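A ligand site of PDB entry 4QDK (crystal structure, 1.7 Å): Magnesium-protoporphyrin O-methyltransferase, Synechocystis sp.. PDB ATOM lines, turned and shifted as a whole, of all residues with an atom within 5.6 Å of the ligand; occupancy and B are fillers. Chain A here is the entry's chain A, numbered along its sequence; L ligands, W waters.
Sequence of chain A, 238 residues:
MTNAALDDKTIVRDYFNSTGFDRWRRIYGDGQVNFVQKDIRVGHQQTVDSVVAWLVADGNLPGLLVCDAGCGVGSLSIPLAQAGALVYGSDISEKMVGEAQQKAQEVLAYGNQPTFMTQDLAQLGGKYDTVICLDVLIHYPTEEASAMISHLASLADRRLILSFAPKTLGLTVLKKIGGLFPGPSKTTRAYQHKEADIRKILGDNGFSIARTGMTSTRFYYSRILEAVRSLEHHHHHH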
ATOM      1  N   LYS A   9      -0.218  -8.648  23.173  1.00  0.00           N
ATOM      2  CA  LYS A   9      -1.002  -7.756  24.021  1.00  0.00           C
ATOM      3  C   LYS A   9      -1.220  -8.325  25.420  1.00  0.00           C
ATOM      4  O   LYS A   9      -1.046  -7.617  26.425  1.00  0.00           O
ATOM      5  CB  LYS A   9      -2.353  -7.442  23.377  1.00  0.00           C
ATOM      6  CG  LYS A   9      -2.290  -6.437  22.243  1.00  0.00           C
ATOM      7  CD  LYS A   9      -3.655  -6.253  21.617  1.00  0.00           C
ATOM      8  CE  LYS A   9      -3.639  -5.187  20.543  1.00  0.00           C
ATOM      9  NZ  LYS A   9      -4.901  -5.208  19.740  1.00  0.00           N
ATOM     10  N   VAL A  12       2.149  -8.359  27.427  1.00  0.00           N
ATOM     11  CA  VAL A  12       2.504  -7.032  27.908  1.00  0.00           C
ATOM     12  C   VAL A  12       1.561  -6.579  29.021  1.00  0.00           C
ATOM     13  O   VAL A  12       1.993  -6.010  30.021  1.00  0.00           O
ATOM     14  CB  VAL A  12       2.508  -5.993  26.766  1.00  0.00           C
ATOM     15  CG1 VAL A  12       2.903  -4.621  27.298  1.00  0.00           C
ATOM     16  CG2 VAL A  12       3.454  -6.423  25.670  1.00  0.00           C
ATOM     17  N   PHE A  16       2.589  -5.612  32.996  1.00  0.00           N
ATOM     18  CA  PHE A  16       2.312  -4.325  33.632  1.00  0.00           C
ATOM     19  C   PHE A  16       1.226  -4.395  34.705  1.00  0.00           C
ATOM     20  O   PHE A  16       0.936  -3.403  35.364  1.00  0.00           O
ATOM     21  CB  PHE A  16       1.988  -3.258  32.585  1.00  0.00           C
ATOM     22  CG  PHE A  16       3.196  -2.731  31.850  1.00  0.00           C
ATOM     23  CD1 PHE A  16       3.521  -3.190  30.590  1.00  0.00           C
ATOM     24  CD2 PHE A  16       4.012  -1.781  32.438  1.00  0.00           C
ATOM     25  CE1 PHE A  16       4.633  -2.716  29.922  1.00  0.00           C
ATOM     26  CE2 PHE A  16       5.125  -1.295  31.777  1.00  0.00           C
ATOM     27  CZ  PHE A  16       5.434  -1.754  30.521  1.00  0.00           C
ATOM     28  N   TYR A  28       8.951   5.478  37.538  1.00  0.00           N
ATOM     29  CA  TYR A  28       8.168   6.649  37.190  1.00  0.00           C
ATOM     30  C   TYR A  28       7.763   7.466  38.414  1.00  0.00           C
ATOM     31  O   TYR A  28       7.221   8.557  38.289  1.00  0.00           O
ATOM     32  CB  TYR A  28       6.923   6.246  36.399  1.00  0.00           C
ATOM     33  CG  TYR A  28       7.183   5.662  35.023  1.00  0.00           C
ATOM     34  CD1 TYR A  28       8.330   6.008  34.315  1.00  0.00           C
ATOM     35  CD2 TYR A  28       6.289   4.774  34.443  1.00  0.00           C
ATOM     36  CE1 TYR A  28       8.570   5.475  33.051  1.00  0.00           C
ATOM     37  CE2 TYR A  28       6.525   4.245  33.188  1.00  0.00           C
ATOM     38  CZ  TYR A  28       7.663   4.597  32.496  1.00  0.00           C
ATOM     39  OH  TYR A  28       7.893   4.073  31.236  1.00  0.00           O
ATOM     40  N   HIS A  44      13.439   9.083  30.852  1.00  0.00           N
ATOM     41  CA  HIS A  44      12.002   9.162  30.621  1.00  0.00           C
ATOM     42  C   HIS A  44      11.457  10.552  30.962  1.00  0.00           C
ATOM     43  O   HIS A  44      10.604  11.086  30.240  1.00  0.00           O
ATOM     44  CB  HIS A  44      11.261   8.100  31.431  1.00  0.00           C
ATOM     45  CG  HIS A  44       9.773   8.204  31.343  1.00  0.00           C
ATOM     46  ND1 HIS A  44       9.006   8.711  32.370  1.00  0.00           N
ATOM     47  CD2 HIS A  44       8.902   7.879  30.358  1.00  0.00           C
ATOM     48  CE1 HIS A  44       7.734   8.689  32.025  1.00  0.00           C
ATOM     49  NE2 HIS A  44       7.642   8.187  30.806  1.00  0.00           N
ATOM     50  N   VAL A  48       9.293  13.097  28.481  1.00  0.00           N
ATOM     51  CA  VAL A  48       8.048  13.725  28.910  1.00  0.00           C
ATOM     52  C   VAL A  48       8.160  15.242  28.851  1.00  0.00           C
ATOM     53  O   VAL A  48       7.292  15.912  28.282  1.00  0.00           O
ATOM     54  CB  VAL A  48       7.647  13.299  30.339  1.00  0.00           C
ATOM     55  CG1 VAL A  48       6.507  14.148  30.855  1.00  0.00           C
ATOM     56  CG2 VAL A  48       7.290  11.822  30.365  1.00  0.00           C
ATOM     57  N   ASP A  68      -3.869  10.515  25.436  1.00  0.00           N
ATOM     58  CA  ASP A  68      -2.615   9.913  25.879  1.00  0.00           C
ATOM     59  C   ASP A  68      -2.802   8.405  25.909  1.00  0.00           C
ATOM     60  O   ASP A  68      -3.373   7.855  26.847  1.00  0.00           O
ATOM     61  CB  ASP A  68      -2.236  10.465  27.261  1.00  0.00           C
ATOM     62  CG  ASP A  68      -0.830  10.048  27.700  1.00  0.00           C
ATOM     63  OD1 ASP A  68      -0.128   9.397  26.908  1.00  0.00           O
ATOM     64  OD2 ASP A  68      -0.436  10.390  28.838  1.00  0.00           O
ATOM     65  N   ALA A  69      -2.357   7.732  24.851  1.00  0.00           N
ATOM     66  CA  ALA A  69      -2.575   6.303  24.681  1.00  0.00           C
ATOM     67  C   ALA A  69      -1.425   5.475  25.252  1.00  0.00           C
ATOM     68  O   ALA A  69      -0.278   5.611  24.838  1.00  0.00           O
ATOM     69  CB  ALA A  69      -2.791   5.956  23.208  1.00  0.00           C
ATOM     70  N   GLY A  70      -1.740   4.608  26.217  1.00  0.00           N
ATOM     71  CA  GLY A  70      -0.727   3.884  26.964  1.00  0.00           C
ATOM     72  C   GLY A  70      -0.117   4.808  28.002  1.00  0.00           C
ATOM     73  O   GLY A  70       1.103   4.915  28.122  1.00  0.00           O
ATOM     74  N   CYS A  71      -0.989   5.479  28.759  1.00  0.00           N
ATOM     75  CA  CYS A  71      -0.592   6.588  29.606  1.00  0.00           C
ATOM     76  C   CYS A  71       0.251   6.205  30.823  1.00  0.00           C
ATOM     77  O   CYS A  71       0.813   7.072  31.491  1.00  0.00           O
ATOM     78  CB  CYS A  71      -1.826   7.360  30.068  1.00  0.00           C
ATOM     79  SG  CYS A  71      -2.959   6.411  31.097  1.00  0.00           S
ATOM     80  N   GLY A  72       0.328   4.903  31.122  1.00  0.00           N
ATOM     81  CA  GLY A  72       1.059   4.443  32.288  1.00  0.00           C
ATOM     82  C   GLY A  72       0.495   5.040  33.564  1.00  0.00           C
ATOM     83  O   GLY A  72      -0.717   5.035  33.776  1.00  0.00           O
ATOM     84  N   VAL A  73       1.368   5.569  34.412  1.00  0.00           N
ATOM     85  CA  VAL A  73       0.936   6.190  35.663  1.00  0.00           C
ATOM     86  C   VAL A  73       0.660   7.684  35.497  1.00  0.00           C
ATOM     87  O   VAL A  73       0.613   8.426  36.470  1.00  0.00           O
ATOM     88  CB  VAL A  73       1.968   5.965  36.785  1.00  0.00           C
ATOM     89  CG1 VAL A  73       2.103   4.477  37.091  1.00  0.00           C
ATOM     90  CG2 VAL A  73       3.306   6.574  36.418  1.00  0.00           C
ATOM     91  N   SER A  75       2.463   9.991  33.757  1.00  0.00           N
ATOM     92  CA  SER A  75       3.649  10.851  33.786  1.00  0.00           C
ATOM     93  C   SER A  75       3.537  12.042  32.823  1.00  0.00           C
ATOM     94  O   SER A  75       4.077  13.113  33.105  1.00  0.00           O
ATOM     95  CB  SER A  75       4.904  10.048  33.453  1.00  0.00           C
ATOM     96  OG  SER A  75       5.160   9.075  34.453  1.00  0.00           O
ATOM     97  N   LEU A  76       2.833  11.842  31.721  1.00  0.00           N
ATOM     98  CA  LEU A  76       2.629  12.889  30.731  1.00  0.00           C
ATOM     99  C   LEU A  76       1.245  13.518  30.863  1.00  0.00           C
ATOM    100  O   LEU A  76       1.088  14.728  30.664  1.00  0.00           O
ATOM    101  CB  LEU A  76       2.813  12.340  29.315  1.00  0.00           C
ATOM    102  CG  LEU A  76       2.455  13.282  28.167  1.00  0.00           C
ATOM    103  CD1 LEU A  76       3.482  14.399  28.028  1.00  0.00           C
ATOM    104  CD2 LEU A  76       2.298  12.516  26.861  1.00  0.00           C
ATOM    105  N   SER A  90      -5.478   6.612  28.607  1.00  0.00           N
ATOM    106  CA  SER A  90      -5.890   5.217  28.632  1.00  0.00           C
ATOM    107  C   SER A  90      -4.688   4.296  28.638  1.00  0.00           C
ATOM    108  O   SER A  90      -3.633   4.647  28.141  1.00  0.00           O
ATOM    109  CB  SER A  90      -6.807   4.895  27.445  1.00  0.00           C
ATOM    110  OG  SER A  90      -6.187   5.220  26.226  1.00  0.00           O
ATOM    111  N   ASP A  91      -4.864   3.111  29.214  1.00  0.00           N
ATOM    112  CA  ASP A  91      -3.800   2.119  29.282  1.00  0.00           C
ATOM    113  C   ASP A  91      -4.406   0.724  29.339  1.00  0.00           C
ATOM    114  O   ASP A  91      -5.492   0.550  29.882  1.00  0.00           O
ATOM    115  CB  ASP A  91      -2.915   2.365  30.506  1.00  0.00           C
ATOM    116  CG  ASP A  91      -1.582   1.661  30.400  1.00  0.00           C
ATOM    117  OD1 ASP A  91      -1.535   0.424  30.577  1.00  0.00           O
ATOM    118  OD2 ASP A  91      -0.559   2.350  30.162  1.00  0.00           O
ATOM    119  N   ILE A  92      -3.704  -0.250  28.789  1.00  0.00           N
ATOM    120  CA  ILE A  92      -4.207  -1.623  28.760  1.00  0.00           C
ATOM    121  C   ILE A  92      -4.174  -2.238  30.162  1.00  0.00           C
ATOM    122  O   ILE A  92      -4.869  -3.224  30.432  1.00  0.00           O
ATOM    123  CB  ILE A  92      -3.393  -2.499  27.778  1.00  0.00           C
ATOM    124  CG1 ILE A  92      -4.180  -3.755  27.393  1.00  0.00           C
ATOM    125  CG2 ILE A  92      -2.036  -2.854  28.358  1.00  0.00           C
ATOM    126  CD1 ILE A  92      -3.594  -4.511  26.214  1.00  0.00           C
ATOM    127  N   SER A  93      -3.397  -1.634  31.052  1.00  0.00           N
ATOM    128  CA  SER A  93      -3.194  -2.165  32.402  1.00  0.00           C
ATOM    129  C   SER A  93      -4.031  -1.425  33.447  1.00  0.00           C
ATOM    130  O   SER A  93      -3.856  -0.231  33.662  1.00  0.00           O
ATOM    131  CB  SER A  93      -1.708  -2.070  32.781  1.00  0.00           C
ATOM    132  OG  SER A  93      -1.533  -2.186  34.184  1.00  0.00           O
ATOM    133  N   MET A  96      -1.859   0.195  36.180  1.00  0.00           N
ATOM    134  CA  MET A  96      -1.295   1.477  35.765  1.00  0.00           C
ATOM    135  C   MET A  96      -2.346   2.584  35.813  1.00  0.00           C
ATOM    136  O   MET A  96      -2.073   3.684  36.281  1.00  0.00           O
ATOM    137  CB  MET A  96      -0.681   1.366  34.366  1.00  0.00           C
ATOM    138  CG  MET A  96       0.571   0.509  34.300  1.00  0.00           C
ATOM    139  SD  MET A  96       1.888   1.208  35.312  1.00  0.00           S
ATOM    140  CE  MET A  96       3.137  -0.054  35.186  1.00  0.00           C
ATOM    141  N   GLN A 119      -8.072   0.466  28.786  1.00  0.00           N
ATOM    142  CA  GLN A 119      -8.435   0.181  27.405  1.00  0.00           C
ATOM    143  C   GLN A 119      -7.203  -0.122  26.549  1.00  0.00           C
ATOM    144  O   GLN A 119      -6.186   0.551  26.657  1.00  0.00           O
ATOM    145  CB  GLN A 119      -9.176   1.376  26.807  1.00  0.00           C
ATOM    146  CG  GLN A 119      -9.716   1.168  25.401  1.00  0.00           C
ATOM    147  CD  GLN A 119     -11.016   0.410  25.371  1.00  0.00           C
ATOM    148  OE1 GLN A 119     -11.102  -0.729  25.845  1.00  0.00           O
ATOM    149  NE2 GLN A 119     -12.053   1.034  24.816  1.00  0.00           N
ATOM    150  N   ASP A 120      -7.320  -1.145  25.706  1.00  0.00           N
ATOM    151  CA  ASP A 120      -6.340  -1.413  24.672  1.00  0.00           C
ATOM    152  C   ASP A 120      -6.446  -0.277  23.650  1.00  0.00           C
ATOM    153  O   ASP A 120      -7.538   0.021  23.156  1.00  0.00           O
ATOM    154  CB  ASP A 120      -6.641  -2.766  24.026  1.00  0.00           C
ATOM    155  CG  ASP A 120      -5.768  -3.060  22.818  1.00  0.00           C
ATOM    156  OD1 ASP A 120      -4.686  -2.458  22.666  1.00  0.00           O
ATOM    157  OD2 ASP A 120      -6.184  -3.926  22.011  1.00  0.00           O
ATOM    158  N   LEU A 121      -5.324   0.374  23.346  1.00  0.00           N
ATOM    159  CA  LEU A 121      -5.326   1.527  22.454  1.00  0.00           C
ATOM    160  C   LEU A 121      -5.907   1.198  21.073  1.00  0.00           C
ATOM    161  O   LEU A 121      -6.408   2.078  20.374  1.00  0.00           O
ATOM    162  CB  LEU A 121      -3.934   2.151  22.334  1.00  0.00           C
ATOM    163  CG  LEU A 121      -2.770   1.334  21.782  1.00  0.00           C
ATOM    164  CD1 LEU A 121      -2.703   1.402  20.260  1.00  0.00           C
ATOM    165  CD2 LEU A 121      -1.454   1.788  22.387  1.00  0.00           C
ATOM    166  N   ALA A 122      -5.828  -0.066  20.683  1.00  0.00           N
ATOM    167  CA  ALA A 122      -6.356  -0.502  19.393  1.00  0.00           C
ATOM    168  C   ALA A 122      -7.884  -0.418  19.352  1.00  0.00           C
ATOM    169  O   ALA A 122      -8.487  -0.418  18.285  1.00  0.00           O
ATOM    170  CB  ALA A 122      -5.895  -1.915  19.077  1.00  0.00           C
ATOM    171  N   CYS A 133       1.504   8.798  21.981  1.00  0.00           N
ATOM    172  CA  CYS A 133       1.852   7.446  22.402  1.00  0.00           C
ATOM    173  C   CYS A 133       3.349   7.356  22.679  1.00  0.00           C
ATOM    174  O   CYS A 133       4.154   7.225  21.753  1.00  0.00           O
ATOM    175  CB  CYS A 133       1.449   6.436  21.325  1.00  0.00           C
ATOM    176  SG  CYS A 133       1.620   4.713  21.821  1.00  0.00           S
ATOM    177  N   LEU A 134       3.720   7.445  23.950  1.00  0.00           N
ATOM    178  CA  LEU A 134       5.130   7.460  24.344  1.00  0.00           C
ATOM    179  C   LEU A 134       5.593   6.153  24.985  1.00  0.00           C
ATOM    180  O   LEU A 134       4.955   5.630  25.902  1.00  0.00           O
ATOM    181  CB  LEU A 134       5.413   8.618  25.304  1.00  0.00           C
ATOM    182  CG  LEU A 134       5.131  10.046  24.839  1.00  0.00           C
ATOM    183  CD1 LEU A 134       5.544  11.061  25.909  1.00  0.00           C
ATOM    184  CD2 LEU A 134       5.837  10.332  23.513  1.00  0.00           C
ATOM    185  N   ASP A 135       6.713   5.637  24.485  1.00  0.00           N
ATOM    186  CA  ASP A 135       7.388   4.470  25.062  1.00  0.00           C
ATOM    187  C   ASP A 135       6.486   3.243  25.200  1.00  0.00           C
ATOM    188  O   ASP A 135       6.603   2.481  26.168  1.00  0.00           O
ATOM    189  CB  ASP A 135       8.030   4.828  26.416  1.00  0.00           C
ATOM    190  CG  ASP A 135       9.120   5.881  26.286  1.00  0.00           C
ATOM    191  OD1 ASP A 135       9.541   6.171  25.145  1.00  0.00           O
ATOM    192  OD2 ASP A 135       9.568   6.411  27.320  1.00  0.00           O
ATOM    193  N   VAL A 136       5.594   3.061  24.233  1.00  0.00           N
ATOM    194  CA  VAL A 136       4.686   1.917  24.218  1.00  0.00           C
ATOM    195  C   VAL A 136       5.063   0.944  23.098  1.00  0.00           C
ATOM    196  O   VAL A 136       5.013  -0.281  23.256  1.00  0.00           O
ATOM    197  CB  VAL A 136       3.227   2.358  24.016  1.00  0.00           C
ATOM    198  CG1 VAL A 136       2.304   1.153  23.885  1.00  0.00           C
ATOM    199  CG2 VAL A 136       2.776   3.263  25.159  1.00  0.00           C
ATOM    200  N   HIS A 139       7.258  -2.412  22.974  1.00  0.00           N
ATOM    201  CA  HIS A 139       6.743  -3.709  23.408  1.00  0.00           C
ATOM    202  C   HIS A 139       6.111  -4.525  22.281  1.00  0.00           C
ATOM    203  O   HIS A 139       5.554  -5.594  22.524  1.00  0.00           O
ATOM    204  CB  HIS A 139       5.729  -3.519  24.537  1.00  0.00           C
ATOM    205  CG  HIS A 139       6.281  -2.807  25.734  1.00  0.00           C
ATOM    206  ND1 HIS A 139       7.216  -3.370  26.568  1.00  0.00           N
ATOM    207  CD2 HIS A 139       6.047  -1.564  26.219  1.00  0.00           C
ATOM    208  CE1 HIS A 139       7.522  -2.510  27.523  1.00  0.00           C
ATOM    209  NE2 HIS A 139       6.823  -1.409  27.339  1.00  0.00           N
ATOM    210  N   TYR A 140       6.197  -4.020  21.054  1.00  0.00           N
ATOM    211  CA  TYR A 140       5.580  -4.708  19.922  1.00  0.00           C
ATOM    212  C   TYR A 140       6.485  -4.720  18.692  1.00  0.00           C
ATOM    213  O   TYR A 140       7.187  -3.753  18.432  1.00  0.00           O
ATOM    214  CB  TYR A 140       4.234  -4.048  19.575  1.00  0.00           C
ATOM    215  CG  TYR A 140       3.242  -4.067  20.712  1.00  0.00           C
ATOM    216  CD1 TYR A 140       2.363  -5.122  20.880  1.00  0.00           C
ATOM    217  CD2 TYR A 140       3.174  -3.013  21.627  1.00  0.00           C
ATOM    218  CE1 TYR A 140       1.455  -5.153  21.922  1.00  0.00           C
ATOM    219  CE2 TYR A 140       2.265  -3.031  22.664  1.00  0.00           C
ATOM    220  CZ  TYR A 140       1.406  -4.101  22.812  1.00  0.00           C
ATOM    221  OH  TYR A 140       0.501  -4.123  23.841  1.00  0.00           O
ATOM    222  N   MET A 148      -1.115  -0.455  15.079  1.00  0.00           N
ATOM    223  CA  MET A 148      -1.346   0.429  16.212  1.00  0.00           C
ATOM    224  C   MET A 148      -1.271   1.893  15.811  1.00  0.00           C
ATOM    225  O   MET A 148      -2.150   2.680  16.152  1.00  0.00           O
ATOM    226  CB  MET A 148      -0.351   0.131  17.345  1.00  0.00           C
ATOM    227  CG  MET A 148      -0.519  -1.264  17.946  1.00  0.00           C
ATOM    228  SD  MET A 148       0.820  -1.717  19.064  1.00  0.00           S
ATOM    229  CE  MET A 148       0.576  -0.560  20.407  1.00  0.00           C
HETATM  230  N1  LIG L   1       3.338   6.402  28.043  1.00  0.00           N
HETATM  231  C1  LIG L   1       3.629   6.322  29.468  1.00  0.00           C
HETATM  232  C2  LIG L   1       3.811   4.883  29.933  1.00  0.00           C
HETATM  233  C3  LIG L   1       4.869   4.091  29.163  1.00  0.00           C
HETATM  234  S1  LIG L   1       5.156   2.462  29.908  1.00  0.00           S
HETATM  235  C4  LIG L   1       4.876   7.128  29.797  1.00  0.00           C
HETATM  236  O1  LIG L   1       5.062   7.582  30.928  1.00  0.00           O
HETATM  237  O2  LIG L   1       5.722   7.357  28.932  1.00  0.00           O
HETATM  238  C5  LIG L   1       4.233   1.650  28.583  1.00  0.00           C
HETATM  239  C6  LIG L   1       2.750   1.513  28.922  1.00  0.00           C
HETATM  240  O3  LIG L   1       2.033   1.108  27.762  1.00  0.00           O
HETATM  241  C7  LIG L   1       2.475   0.460  29.990  1.00  0.00           C
HETATM  242  O4  LIG L   1       1.787   1.081  31.050  1.00  0.00           O
HETATM  243  C8  LIG L   1       1.556  -0.546  29.324  1.00  0.00           C
HETATM  244  O5  LIG L   1       0.540  -1.012  30.181  1.00  0.00           O
HETATM  245  C9  LIG L   1       0.986   0.257  28.168  1.00  0.00           C
HETATM  246  N2  LIG L   1       0.522  -0.564  27.035  1.00  0.00           N
HETATM  247  C10 LIG L   1       1.154  -1.636  26.474  1.00  0.00           C
HETATM  248  N3  LIG L   1       0.389  -2.094  25.452  1.00  0.00           N
HETATM  249  C11 LIG L   1      -0.716  -1.324  25.364  1.00  0.00           C
HETATM  250  C12 LIG L   1      -1.816  -1.357  24.518  1.00  0.00           C
HETATM  251  N4  LIG L   1      -1.907  -2.271  23.564  1.00  0.00           N
HETATM  252  N5  LIG L   1      -2.815  -0.420  24.670  1.00  0.00           N
HETATM  253  C13 LIG L   1      -2.723   0.544  25.654  1.00  0.00           C
HETATM  254  N6  LIG L   1      -1.636   0.561  26.499  1.00  0.00           N
HETATM  255  C14 LIG L   1      -0.641  -0.360  26.351  1.00  0.00           C
HETATM  256  O   HOH W   1       8.120   1.261  30.481  1.00  0.00           O
HETATM  257  O   HOH W   2       2.582   9.211  28.138  1.00  0.00           O
HETATM  258  O   HOH W   3       3.517   7.097  33.195  1.00  0.00           O
HETATM  259  O   HOH W   4       1.582   7.234  25.761  1.00  0.00           O
HETATM  260  O   HOH W   5      -4.887   2.870  25.712  1.00  0.00           O
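Water W3 lies within hydrogen-bond range of O1 of the ligand (2.8 Å), OG of Ser 75 (2.9 Å), N of Val 73 (2.9 Å) and O of Cys 71 (3.2 Å). Water W2 lies within hydrogen-bond range of a nitrogen (N1) of the ligand (2.9 Å) and the side-chain carboxylate of Asp 68 (3.0 Å). Water W5 lies within hydrogen-bond range of the side-chain hydroxyl of Ser 90, the backbone carbonyl oxygen of Gln 119 and the backbone NH of Leu 121. Water W1 bridges OH of Tyr 28 (2.9 Å) and S1 of the ligand (3.2 Å).
Merely in contact with the ligand: Val 136 (3.5 Å), Asp 135 (3.5 Å), Met 96 (3.5 Å), Phe 16 (3.5 Å), Ser 75 (3.5 Å), Cys 71 (3.5 Å), Val 12 (3.6 Å), Ser 93 (3.6 Å), Gln 119 (3.6 Å) and Gly 72 (3.6 Å). Hydrophobic or aromatic side chains that line the ligand: Val 12, Phe 16, Tyr 28, His 44, Ile 92, Met 96, Leu 121, Leu 134, Val 136 and Tyr 140. The nearest printed residue that does not touch the ligand is His 139 (4.2 Å).
The side-chain carboxylate (OD2) of Asp 91 is in hydrogen-bond range of the backbone NH (N) of Cys 71. The backbone NH of Gln 119 sits at hydrogen-bond distance from the backbone carbonyl oxygen of Asp 91, at 2.8 Å. OD2 of Asp 91 lies within hydrogen-bond range of N of Gly 72 (2.9 Å). N of Gly 70 is in hydrogen-bond range of O of Ser 90 (2.7 Å). The backbone carbonyl oxygen (O) of Gln 119 sits at hydrogen-bond distance from the backbone NH (N) of Ile 92, at 3.4 Å. The side-chain hydroxyl of Ser 93 lies within hydrogen-bond range of the backbone NH of Met 96 (3.1 Å). The backbone carbonyl oxygen of Phe 16 is in hydrogen-bond range of the side-chain hydroxyl of Ser 93 (3.0 Å). The backbone NH of Cys 71 lies within hydrogen-bond range of the backbone carbonyl oxygen of Ser 90, 2.8 Å away.
The side-chain carboxylate (OD1) of Asp 91 lies within hydrogen-bond range of an oxygen (O5) of the ligand, at 2.6 Å. The side-chain hydroxyl (OH) of Tyr 140 sits at hydrogen-bond distance from a nitrogen (N3) of the ligand, at 2.6 Å. A ring nitrogen (NE2) of His 44 lies within hydrogen-bond range of an oxygen (O1) of the ligand (2.7 Å). N1 of the ligand is in hydrogen-bond range of O of Gly 70 (2.7 Å). The backbone carbonyl oxygen (O) of Leu 134 lies within hydrogen-bond range of a nitrogen (N1) of the ligand, at 2.8 Å. N4 of the ligand is in hydrogen-bond range of OD1 of Asp 120 (2.9 Å). The backbone NH (N) of Leu 121 lies within hydrogen-bond range of a nitrogen (N5) of the ligand (2.9 Å). N6 of the ligand is in hydrogen-bond range of N of Ile 92. The side-chain hydroxyl of Tyr 28 sits close to a sulfur (S1) of the ligand, at 3.4 Å.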
